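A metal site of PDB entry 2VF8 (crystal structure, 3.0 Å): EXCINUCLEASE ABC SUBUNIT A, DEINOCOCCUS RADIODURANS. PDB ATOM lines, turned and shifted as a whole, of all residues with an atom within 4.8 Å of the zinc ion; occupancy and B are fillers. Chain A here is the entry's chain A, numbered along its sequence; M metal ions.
The side-chain sulfur (SG) of Cys 154 sits close to the backbone NH (N) of Gly 158, 3.1 Å away. The backbone NH (N) of Cys 287 lies close to the backbone carbonyl oxygen (O) of Gly 158 (3.1 Å). N of Glu 153 sits close to SG of Cys 151 (3.7 Å).
Within 4 Å of the zinc ion: Cys 151, Cys 154, Cys 287 and Cys 290.
SG of Cys 287 binds the zinc ion, at 2.0 Å. SG of Cys 151 binds the zinc ion, at 2.1 Å. SG of Cys 290 is bound to the zinc ion, at 2.1 Å. SG of Cys 154 binds the zinc ion (2.5 Å). The zinc ion has four donor atoms within binding distance.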
ATOM      1  N   CYS A 151      26.473 -13.145   0.457  1.00  0.00           N
ATOM      2  CA  CYS A 151      27.487 -14.159   0.132  1.00  0.00           C
ATOM      3  C   CYS A 151      28.578 -13.490  -0.669  1.00  0.00           C
ATOM      4  O   CYS A 151      28.289 -12.768  -1.636  1.00  0.00           O
ATOM      5  CB  CYS A 151      26.916 -15.356  -0.654  1.00  0.00           C
ATOM      6  SG  CYS A 151      27.463 -15.519  -2.353  1.00  0.00           S
ATOM      7  N   GLU A 153      30.934 -14.179  -2.805  1.00  0.00           N
ATOM      8  CA  GLU A 153      31.127 -14.376  -4.266  1.00  0.00           C
ATOM      9  C   GLU A 153      30.215 -13.488  -5.149  1.00  0.00           C
ATOM     10  O   GLU A 153      30.708 -12.618  -5.872  1.00  0.00           O
ATOM     11  CB  GLU A 153      31.013 -15.870  -4.653  1.00  0.00           C
ATOM     12  CG  GLU A 153      31.173 -16.152  -6.165  1.00  0.00           C
ATOM     13  CD  GLU A 153      31.806 -17.536  -6.503  1.00  0.00           C
ATOM     14  OE1 GLU A 153      32.583 -17.620  -7.479  1.00  0.00           O
ATOM     15  OE2 GLU A 153      31.530 -18.540  -5.802  1.00  0.00           O
ATOM     16  N   CYS A 154      28.912 -13.690  -5.095  1.00  0.00           N
ATOM     17  CA  CYS A 154      27.996 -12.912  -5.949  1.00  0.00           C
ATOM     18  C   CYS A 154      27.741 -11.514  -5.419  1.00  0.00           C
ATOM     19  O   CYS A 154      27.213 -10.669  -6.142  1.00  0.00           O
ATOM     20  CB  CYS A 154      26.657 -13.623  -6.063  1.00  0.00           C
ATOM     21  SG  CYS A 154      25.871 -13.887  -4.482  1.00  0.00           S
ATOM     22  N   GLY A 158      23.495 -12.904  -6.154  1.00  0.00           N
ATOM     23  CA  GLY A 158      23.022 -14.281  -6.301  1.00  0.00           C
ATOM     24  C   GLY A 158      23.409 -14.854  -7.643  1.00  0.00           C
ATOM     25  O   GLY A 158      23.420 -16.071  -7.833  1.00  0.00           O
ATOM     26  N   CYS A 287      25.342 -18.089  -9.220  1.00  0.00           N
ATOM     27  CA  CYS A 287      26.399 -18.217  -8.218  1.00  0.00           C
ATOM     28  C   CYS A 287      26.554 -19.664  -7.694  1.00  0.00           C
ATOM     29  O   CYS A 287      25.575 -20.275  -7.290  1.00  0.00           O
ATOM     30  CB  CYS A 287      26.050 -17.274  -7.076  1.00  0.00           C
ATOM     31  SG  CYS A 287      27.263 -17.117  -5.854  1.00  0.00           S
ATOM     32  N   LEU A 289      28.274 -20.714  -5.103  1.00  0.00           N
ATOM     33  CA  LEU A 289      28.516 -20.735  -3.652  1.00  0.00           C
ATOM     34  C   LEU A 289      27.193 -20.882  -2.921  1.00  0.00           C
ATOM     35  O   LEU A 289      26.955 -21.862  -2.213  1.00  0.00           O
ATOM     36  CB  LEU A 289      29.200 -19.423  -3.209  1.00  0.00           C
ATOM     37  CG  LEU A 289      29.710 -19.107  -1.783  1.00  0.00           C
ATOM     38  CD1 LEU A 289      28.613 -19.093  -0.688  1.00  0.00           C
ATOM     39  CD2 LEU A 289      30.883 -20.011  -1.387  1.00  0.00           C
ATOM     40  N   CYS A 290      26.313 -19.909  -3.143  1.00  0.00           N
ATOM     41  CA  CYS A 290      25.086 -19.718  -2.383  1.00  0.00           C
ATOM     42  C   CYS A 290      23.863 -20.280  -3.120  1.00  0.00           C
ATOM     43  O   CYS A 290      22.737 -20.230  -2.600  1.00  0.00           O
ATOM     44  CB  CYS A 290      24.891 -18.232  -2.147  1.00  0.00           C
ATOM     45  SG  CYS A 290      24.842 -17.358  -3.700  1.00  0.00           S
HETATM   46 ZN    ZN M   1      26.635 -16.251  -4.126  1.00  0.00          ZN
